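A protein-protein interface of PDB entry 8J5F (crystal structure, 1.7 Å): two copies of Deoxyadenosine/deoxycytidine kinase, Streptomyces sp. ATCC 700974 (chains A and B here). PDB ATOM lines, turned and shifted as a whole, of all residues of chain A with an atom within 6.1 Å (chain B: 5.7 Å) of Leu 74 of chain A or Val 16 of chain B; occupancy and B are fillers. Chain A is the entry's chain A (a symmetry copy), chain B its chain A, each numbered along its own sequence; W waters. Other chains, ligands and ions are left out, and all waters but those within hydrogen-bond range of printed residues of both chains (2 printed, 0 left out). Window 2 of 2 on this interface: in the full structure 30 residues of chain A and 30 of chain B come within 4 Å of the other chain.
OD2 of Asp 100 of chain B sits at hydrogen-bond distance from OH of Tyr 71 of chain A (2.8 Å).
O of Asp 15 of chain B lies within hydrogen-bond range of NH2 of Arg 104 of chain B (2.8 Å).
The guanidinium group of Arg 104 of chain B sits at hydrogen-bond distance from the backbone carbonyl oxygen of Gly 17 of chain B, 2.7 Å away.
The guanidinium group (NH2) of Arg 104 of chain B is in salt-bridge range of the side-chain carboxylate (OD1) of Asp 100 of chain B (3.0 Å).
NH1 of Arg 70 of chain A touches CD2 of Tyr 14 of chain B (3.4 Å).
Val 16 of chain B touches Arg 70 of chain A.
CD1 of Tyr 14 of chain B touches CZ of Tyr 71 of chain A, at 3.4 Å.
CD2 of Leu 74 of chain A touches O of Val 16 of chain B (3.8 Å).
Leu 74 of chain A touches Arg 104 of chain B.
Asp 100 of chain B touches Phe 82 of chain A (N to CZ, 3.9 Å).
CE1 of Phe 82 of chain A touches CD of Arg 104 of chain B, 3.9 Å away.
Of chain B, only Val 16 and Arg 104 come within 4 Å of Leu 74 of chain A.
Of the printed residues of chain B, Phe 82 of chain A touches Asp 100 (3.9 Å) and Arg 104 (3.9 Å).
Printed residues of chain A within 4 Å of Tyr 14 of chain B: Arg 70 (3.4 Å) and Tyr 71 (3.4 Å).
Printed residues of chain A within 4 Å of Asp 100 of chain B: Tyr 71 (2.8 Å) and Phe 82 (3.9 Å).
The nearest printed residue of chain A that does not touch Val 16 of chain B is Tyr 71 of chain A (4.01 Å).
Of the 7 printed residues of chain B, 4 touch a printed residue of chain A.
Among the printed residues, 8 pairs touch across the chains.
Among the printed residues, no Asp or Glu carboxylate lies within 4 Å of a Lys or Arg side-chain nitrogen of the other chain.
No position is printed for both chains.
Of the 8 pairs that touch across the chains among the printed residues, none has its exchanged pair printed and touching as well.
Water W2 bridges the backbone carbonyl oxygen (O) of Tyr 14 of chain B (2.8 Å) and the backbone carbonyl oxygen (O) of Arg 70 of chain A (2.8 Å).
Water W1 lies within hydrogen-bond range of OG of Ser 77 of chain A (2.8 Å) and O of Val 16 of chain B (2.9 Å).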
ATOM      1  N   ARG A  70       6.961  15.852 -36.396  1.00  0.00           N
ATOM      2  CA  ARG A  70       7.150  17.214 -35.896  1.00  0.00           C
ATOM      3  C   ARG A  70       7.591  17.239 -34.432  1.00  0.00           C
ATOM      4  O   ARG A  70       8.278  18.176 -34.000  1.00  0.00           O
ATOM      5  CB  ARG A  70       5.850  17.999 -36.102  1.00  0.00           C
ATOM      6  CG  ARG A  70       5.560  18.239 -37.582  1.00  0.00           C
ATOM      7  CD  ARG A  70       4.377  19.159 -37.854  1.00  0.00           C
ATOM      8  NE  ARG A  70       4.744  20.563 -37.717  1.00  0.00           N
ATOM      9  CZ  ARG A  70       3.913  21.579 -37.909  1.00  0.00           C
ATOM     10  NH1 ARG A  70       2.672  21.386 -38.334  1.00  0.00           N
ATOM     11  NH2 ARG A  70       4.336  22.817 -37.670  1.00  0.00           N
ATOM     12  N   TYR A  71       7.233  16.226 -33.658  1.00  0.00           N
ATOM     13  CA  TYR A  71       7.595  16.171 -32.250  1.00  0.00           C
ATOM     14  C   TYR A  71       8.909  15.419 -31.988  1.00  0.00           C
ATOM     15  O   TYR A  71       9.204  15.109 -30.827  1.00  0.00           O
ATOM     16  CB  TYR A  71       6.467  15.517 -31.454  1.00  0.00           C
ATOM     17  CG  TYR A  71       5.208  16.340 -31.199  1.00  0.00           C
ATOM     18  CD1 TYR A  71       5.264  17.640 -30.715  1.00  0.00           C
ATOM     19  CD2 TYR A  71       3.951  15.759 -31.383  1.00  0.00           C
ATOM     20  CE1 TYR A  71       4.093  18.358 -30.441  1.00  0.00           C
ATOM     21  CE2 TYR A  71       2.777  16.459 -31.113  1.00  0.00           C
ATOM     22  CZ  TYR A  71       2.856  17.755 -30.638  1.00  0.00           C
ATOM     23  OH  TYR A  71       1.688  18.437 -30.367  1.00  0.00           O
ATOM     24  N   LEU A  72       9.697  15.122 -33.031  1.00  0.00           N
ATOM     25  CA  LEU A  72      10.919  14.327 -32.867  1.00  0.00           C
ATOM     26  C   LEU A  72      11.770  14.744 -31.662  1.00  0.00           C
ATOM     27  O   LEU A  72      12.215  13.897 -30.878  1.00  0.00           O
ATOM     28  CB  LEU A  72      11.761  14.429 -34.141  1.00  0.00           C
ATOM     29  CG  LEU A  72      13.098  13.680 -34.114  1.00  0.00           C
ATOM     30  CD1 LEU A  72      12.877  12.181 -33.942  1.00  0.00           C
ATOM     31  CD2 LEU A  72      13.858  13.968 -35.389  1.00  0.00           C
ATOM     32  N   LYS A  73      12.029  16.045 -31.512  1.00  0.00           N
ATOM     33  CA  LYS A  73      12.978  16.487 -30.486  1.00  0.00           C
ATOM     34  C   LYS A  73      12.530  16.153 -29.070  1.00  0.00           C
ATOM     35  O   LYS A  73      13.381  16.036 -28.179  1.00  0.00           O
ATOM     36  CB  LYS A  73      13.203  17.993 -30.594  1.00  0.00           C
ATOM     37  CG  LYS A  73      14.022  18.381 -31.832  1.00  0.00           C
ATOM     38  CD  LYS A  73      14.570  19.786 -31.689  1.00  0.00           C
ATOM     39  CE  LYS A  73      15.284  20.208 -32.954  1.00  0.00           C
ATOM     40  NZ  LYS A  73      15.347  21.696 -33.082  1.00  0.00           N
ATOM     41  N   LEU A  74      11.225  15.993 -28.841  1.00  0.00           N
ATOM     42  CA  LEU A  74      10.743  15.640 -27.512  1.00  0.00           C
ATOM     43  C   LEU A  74      11.108  14.204 -27.138  1.00  0.00           C
ATOM     44  O   LEU A  74      11.186  13.879 -25.947  1.00  0.00           O
ATOM     45  CB  LEU A  74       9.223  15.858 -27.434  1.00  0.00           C
ATOM     46  CG  LEU A  74       8.729  17.312 -27.449  1.00  0.00           C
ATOM     47  CD1 LEU A  74       7.206  17.352 -27.628  1.00  0.00           C
ATOM     48  CD2 LEU A  74       9.125  18.048 -26.184  1.00  0.00           C
ATOM     49  N   MET A  75      11.351  13.339 -28.120  1.00  0.00           N
ATOM     50  CA  MET A  75      11.879  12.024 -27.779  1.00  0.00           C
ATOM     51  C   MET A  75      13.218  12.131 -27.060  1.00  0.00           C
ATOM     52  O   MET A  75      13.535  11.297 -26.203  1.00  0.00           O
ATOM     53  CB  MET A  75      12.042  11.172 -29.033  1.00  0.00           C
ATOM     54  CG  MET A  75      12.617   9.787 -28.726  1.00  0.00           C
ATOM     55  SD  MET A  75      12.249   8.532 -29.932  1.00  0.00           S
ATOM     56  CE  MET A  75      13.169   9.205 -31.326  1.00  0.00           C
ATOM     57  N   PHE A  76      14.015  13.134 -27.398  1.00  0.00           N
ATOM     58  CA  PHE A  76      15.335  13.259 -26.808  1.00  0.00           C
ATOM     59  C   PHE A  76      15.383  14.225 -25.634  1.00  0.00           C
ATOM     60  O   PHE A  76      16.303  14.123 -24.825  1.00  0.00           O
ATOM     61  CB  PHE A  76      16.354  13.683 -27.879  1.00  0.00           C
ATOM     62  CG  PHE A  76      16.445  12.708 -29.026  1.00  0.00           C
ATOM     63  CD1 PHE A  76      16.674  11.349 -28.789  1.00  0.00           C
ATOM     64  CD2 PHE A  76      16.277  13.141 -30.328  1.00  0.00           C
ATOM     65  CE1 PHE A  76      16.733  10.433 -29.855  1.00  0.00           C
ATOM     66  CE2 PHE A  76      16.341  12.241 -31.400  1.00  0.00           C
ATOM     67  CZ  PHE A  76      16.569  10.886 -31.158  1.00  0.00           C
ATOM     68  N   SER A  77      14.412  15.133 -25.500  1.00  0.00           N
ATOM     69  CA  SER A  77      14.393  16.047 -24.367  1.00  0.00           C
ATOM     70  C   SER A  77      13.457  15.604 -23.250  1.00  0.00           C
ATOM     71  O   SER A  77      13.624  16.054 -22.106  1.00  0.00           O
ATOM     72  CB  SER A  77      13.997  17.457 -24.828  1.00  0.00           C
ATOM     73  OG  SER A  77      12.665  17.472 -25.303  1.00  0.00           O
ATOM     74  N   ALA A  78      12.485  14.738 -23.553  1.00  0.00           N
ATOM     75  CA  ALA A  78      11.524  14.224 -22.571  1.00  0.00           C
ATOM     76  C   ALA A  78      11.226  12.753 -22.881  1.00  0.00           C
ATOM     77  O   ALA A  78      10.097  12.367 -23.179  1.00  0.00           O
ATOM     78  CB  ALA A  78      10.230  15.046 -22.580  1.00  0.00           C
ATOM     79  N   SER A  79      12.261  11.912 -22.794  1.00  0.00           N
ATOM     80  CA  SER A  79      12.186  10.574 -23.381  1.00  0.00           C
ATOM     81  C   SER A  79      11.173   9.670 -22.670  1.00  0.00           C
ATOM     82  O   SER A  79      10.521   8.848 -23.326  1.00  0.00           O
ATOM     83  CB  SER A  79      13.577   9.928 -23.397  1.00  0.00           C
ATOM     84  OG  SER A  79      14.062   9.707 -22.078  1.00  0.00           O
ATOM     85  N   ASP A  81       8.375  10.366 -21.645  1.00  0.00           N
ATOM     86  CA  ASP A  81       7.049  10.737 -22.121  1.00  0.00           C
ATOM     87  C   ASP A  81       6.865  10.512 -23.612  1.00  0.00           C
ATOM     88  O   ASP A  81       5.801  10.037 -24.024  1.00  0.00           O
ATOM     89  CB  ASP A  81       6.768  12.203 -21.791  1.00  0.00           C
ATOM     90  CG  ASP A  81       6.783  12.466 -20.293  1.00  0.00           C
ATOM     91  OD1 ASP A  81       6.084  11.733 -19.563  1.00  0.00           O
ATOM     92  OD2 ASP A  81       7.514  13.379 -19.852  1.00  0.00           O
ATOM     93  N   PHE A  82       7.874  10.809 -24.441  1.00  0.00           N
ATOM     94  CA  PHE A  82       7.661  10.787 -25.890  1.00  0.00           C
ATOM     95  C   PHE A  82       8.414   9.698 -26.644  1.00  0.00           C
ATOM     96  O   PHE A  82       8.132   9.509 -27.832  1.00  0.00           O
ATOM     97  CB  PHE A  82       8.002  12.166 -26.490  1.00  0.00           C
ATOM     98  CG  PHE A  82       6.954  13.211 -26.196  1.00  0.00           C
ATOM     99  CD1 PHE A  82       6.928  13.874 -24.973  1.00  0.00           C
ATOM    100  CD2 PHE A  82       5.960  13.489 -27.121  1.00  0.00           C
ATOM    101  CE1 PHE A  82       5.949  14.814 -24.682  1.00  0.00           C
ATOM    102  CE2 PHE A  82       4.970  14.428 -26.838  1.00  0.00           C
ATOM    103  CZ  PHE A  82       4.963  15.094 -25.614  1.00  0.00           C
ATOM    104  N   ALA A  83       9.335   8.960 -26.013  1.00  0.00           N
ATOM    105  CA  ALA A  83      10.046   7.913 -26.755  1.00  0.00           C
ATOM    106  C   ALA A  83       9.089   6.847 -27.291  1.00  0.00           C
ATOM    107  O   ALA A  83       9.202   6.426 -28.448  1.00  0.00           O
ATOM    108  CB  ALA A  83      11.119   7.267 -25.879  1.00  0.00           C
ATOM    109  N   ILE A  86       6.868   8.334 -30.271  1.00  0.00           N
ATOM    110  CA  ILE A  86       7.691   8.684 -31.430  1.00  0.00           C
ATOM    111  C   ILE A  86       8.288   7.424 -32.068  1.00  0.00           C
ATOM    112  O   ILE A  86       8.415   7.343 -33.295  1.00  0.00           O
ATOM    113  CB  ILE A  86       8.776   9.704 -31.048  1.00  0.00           C
ATOM    114  CG1 ILE A  86       8.138  11.026 -30.603  1.00  0.00           C
ATOM    115  CG2 ILE A  86       9.720   9.952 -32.259  1.00  0.00           C
ATOM    116  CD1 ILE A  86       7.298  11.688 -31.681  1.00  0.00           C
ATOM    117  N   TYR B  14       2.428  22.361 -32.608  1.00  0.00           N
ATOM    118  CA  TYR B  14       3.568  21.444 -32.618  1.00  0.00           C
ATOM    119  C   TYR B  14       4.847  22.098 -32.102  1.00  0.00           C
ATOM    120  O   TYR B  14       5.912  21.986 -32.719  1.00  0.00           O
ATOM    121  CB  TYR B  14       3.766  20.893 -34.038  1.00  0.00           C
ATOM    122  CG  TYR B  14       2.693  19.889 -34.440  1.00  0.00           C
ATOM    123  CD1 TYR B  14       2.732  18.581 -33.976  1.00  0.00           C
ATOM    124  CD2 TYR B  14       1.641  20.256 -35.277  1.00  0.00           C
ATOM    125  CE1 TYR B  14       1.747  17.644 -34.350  1.00  0.00           C
ATOM    126  CE2 TYR B  14       0.654  19.343 -35.645  1.00  0.00           C
ATOM    127  CZ  TYR B  14       0.707  18.041 -35.174  1.00  0.00           C
ATOM    128  OH  TYR B  14      -0.269  17.134 -35.555  1.00  0.00           O
ATOM    129  N   ASP B  15       4.761  22.754 -30.950  1.00  0.00           N
ATOM    130  CA  ASP B  15       5.895  23.421 -30.318  1.00  0.00           C
ATOM    131  C   ASP B  15       6.634  22.424 -29.425  1.00  0.00           C
ATOM    132  O   ASP B  15       6.033  21.844 -28.517  1.00  0.00           O
ATOM    133  CB  ASP B  15       5.381  24.600 -29.491  1.00  0.00           C
ATOM    134  CG  ASP B  15       6.481  25.559 -29.045  1.00  0.00           C
ATOM    135  OD1 ASP B  15       7.647  25.150 -28.922  1.00  0.00           O
ATOM    136  OD2 ASP B  15       6.147  26.732 -28.764  1.00  0.00           O
ATOM    137  N   VAL B  16       7.935  22.235 -29.662  1.00  0.00           N
ATOM    138  CA  VAL B  16       8.724  21.335 -28.817  1.00  0.00           C
ATOM    139  C   VAL B  16       9.450  22.111 -27.716  1.00  0.00           C
ATOM    140  O   VAL B  16      10.259  21.541 -26.973  1.00  0.00           O
ATOM    141  CB  VAL B  16       9.726  20.513 -29.654  1.00  0.00           C
ATOM    142  CG1 VAL B  16       9.000  19.537 -30.589  1.00  0.00           C
ATOM    143  CG2 VAL B  16      10.655  21.429 -30.445  1.00  0.00           C
ATOM    144  N   GLY B  17       9.160  23.414 -27.589  1.00  0.00           N
ATOM    145  CA  GLY B  17       9.785  24.235 -26.567  1.00  0.00           C
ATOM    146  C   GLY B  17       9.177  24.023 -25.192  1.00  0.00           C
ATOM    147  O   GLY B  17       8.271  23.210 -24.989  1.00  0.00           O
ATOM    148  N   PRO B  18       9.674  24.785 -24.214  1.00  0.00           N
ATOM    149  CA  PRO B  18       9.265  24.559 -22.821  1.00  0.00           C
ATOM    150  C   PRO B  18       7.850  25.037 -22.526  1.00  0.00           C
ATOM    151  O   PRO B  18       7.295  25.919 -23.188  1.00  0.00           O
ATOM    152  CB  PRO B  18      10.293  25.364 -22.008  1.00  0.00           C
ATOM    153  CG  PRO B  18      11.408  25.667 -22.968  1.00  0.00           C
ATOM    154  CD  PRO B  18      10.741  25.793 -24.308  1.00  0.00           C
ATOM    155  N   ASP B 100       1.298  16.456 -25.830  1.00  0.00           N
ATOM    156  CA  ASP B 100       2.044  17.712 -25.853  1.00  0.00           C
ATOM    157  C   ASP B 100       1.183  18.894 -25.404  1.00  0.00           C
ATOM    158  O   ASP B 100       1.534  19.608 -24.460  1.00  0.00           O
ATOM    159  CB  ASP B 100       2.599  17.968 -27.253  1.00  0.00           C
ATOM    160  CG  ASP B 100       3.091  19.393 -27.428  1.00  0.00           C
ATOM    161  OD1 ASP B 100       3.993  19.817 -26.673  1.00  0.00           O
ATOM    162  OD2 ASP B 100       2.570  20.090 -28.315  1.00  0.00           O
ATOM    163  N   ARG B 104       1.639  18.097 -21.405  1.00  0.00           N
ATOM    164  CA  ARG B 104       2.950  18.729 -21.232  1.00  0.00           C
ATOM    165  C   ARG B 104       2.837  20.241 -21.104  1.00  0.00           C
ATOM    166  O   ARG B 104       3.473  20.854 -20.231  1.00  0.00           O
ATOM    167  CB  ARG B 104       3.871  18.383 -22.401  1.00  0.00           C
ATOM    168  CG  ARG B 104       5.315  18.857 -22.187  1.00  0.00           C
ATOM    169  CD  ARG B 104       6.170  18.448 -23.382  1.00  0.00           C
ATOM    170  NE  ARG B 104       5.984  19.342 -24.518  1.00  0.00           N
ATOM    171  CZ  ARG B 104       6.663  20.466 -24.688  1.00  0.00           C
ATOM    172  NH1 ARG B 104       7.551  20.874 -23.793  1.00  0.00           N
ATOM    173  NH2 ARG B 104       6.458  21.186 -25.789  1.00  0.00           N
HETATM  174  O   HOH W   1      12.237  19.412 -27.263  1.00  0.00           O
HETATM  175  O   HOH W   2       7.952  20.914 -34.226  1.00  0.00           O
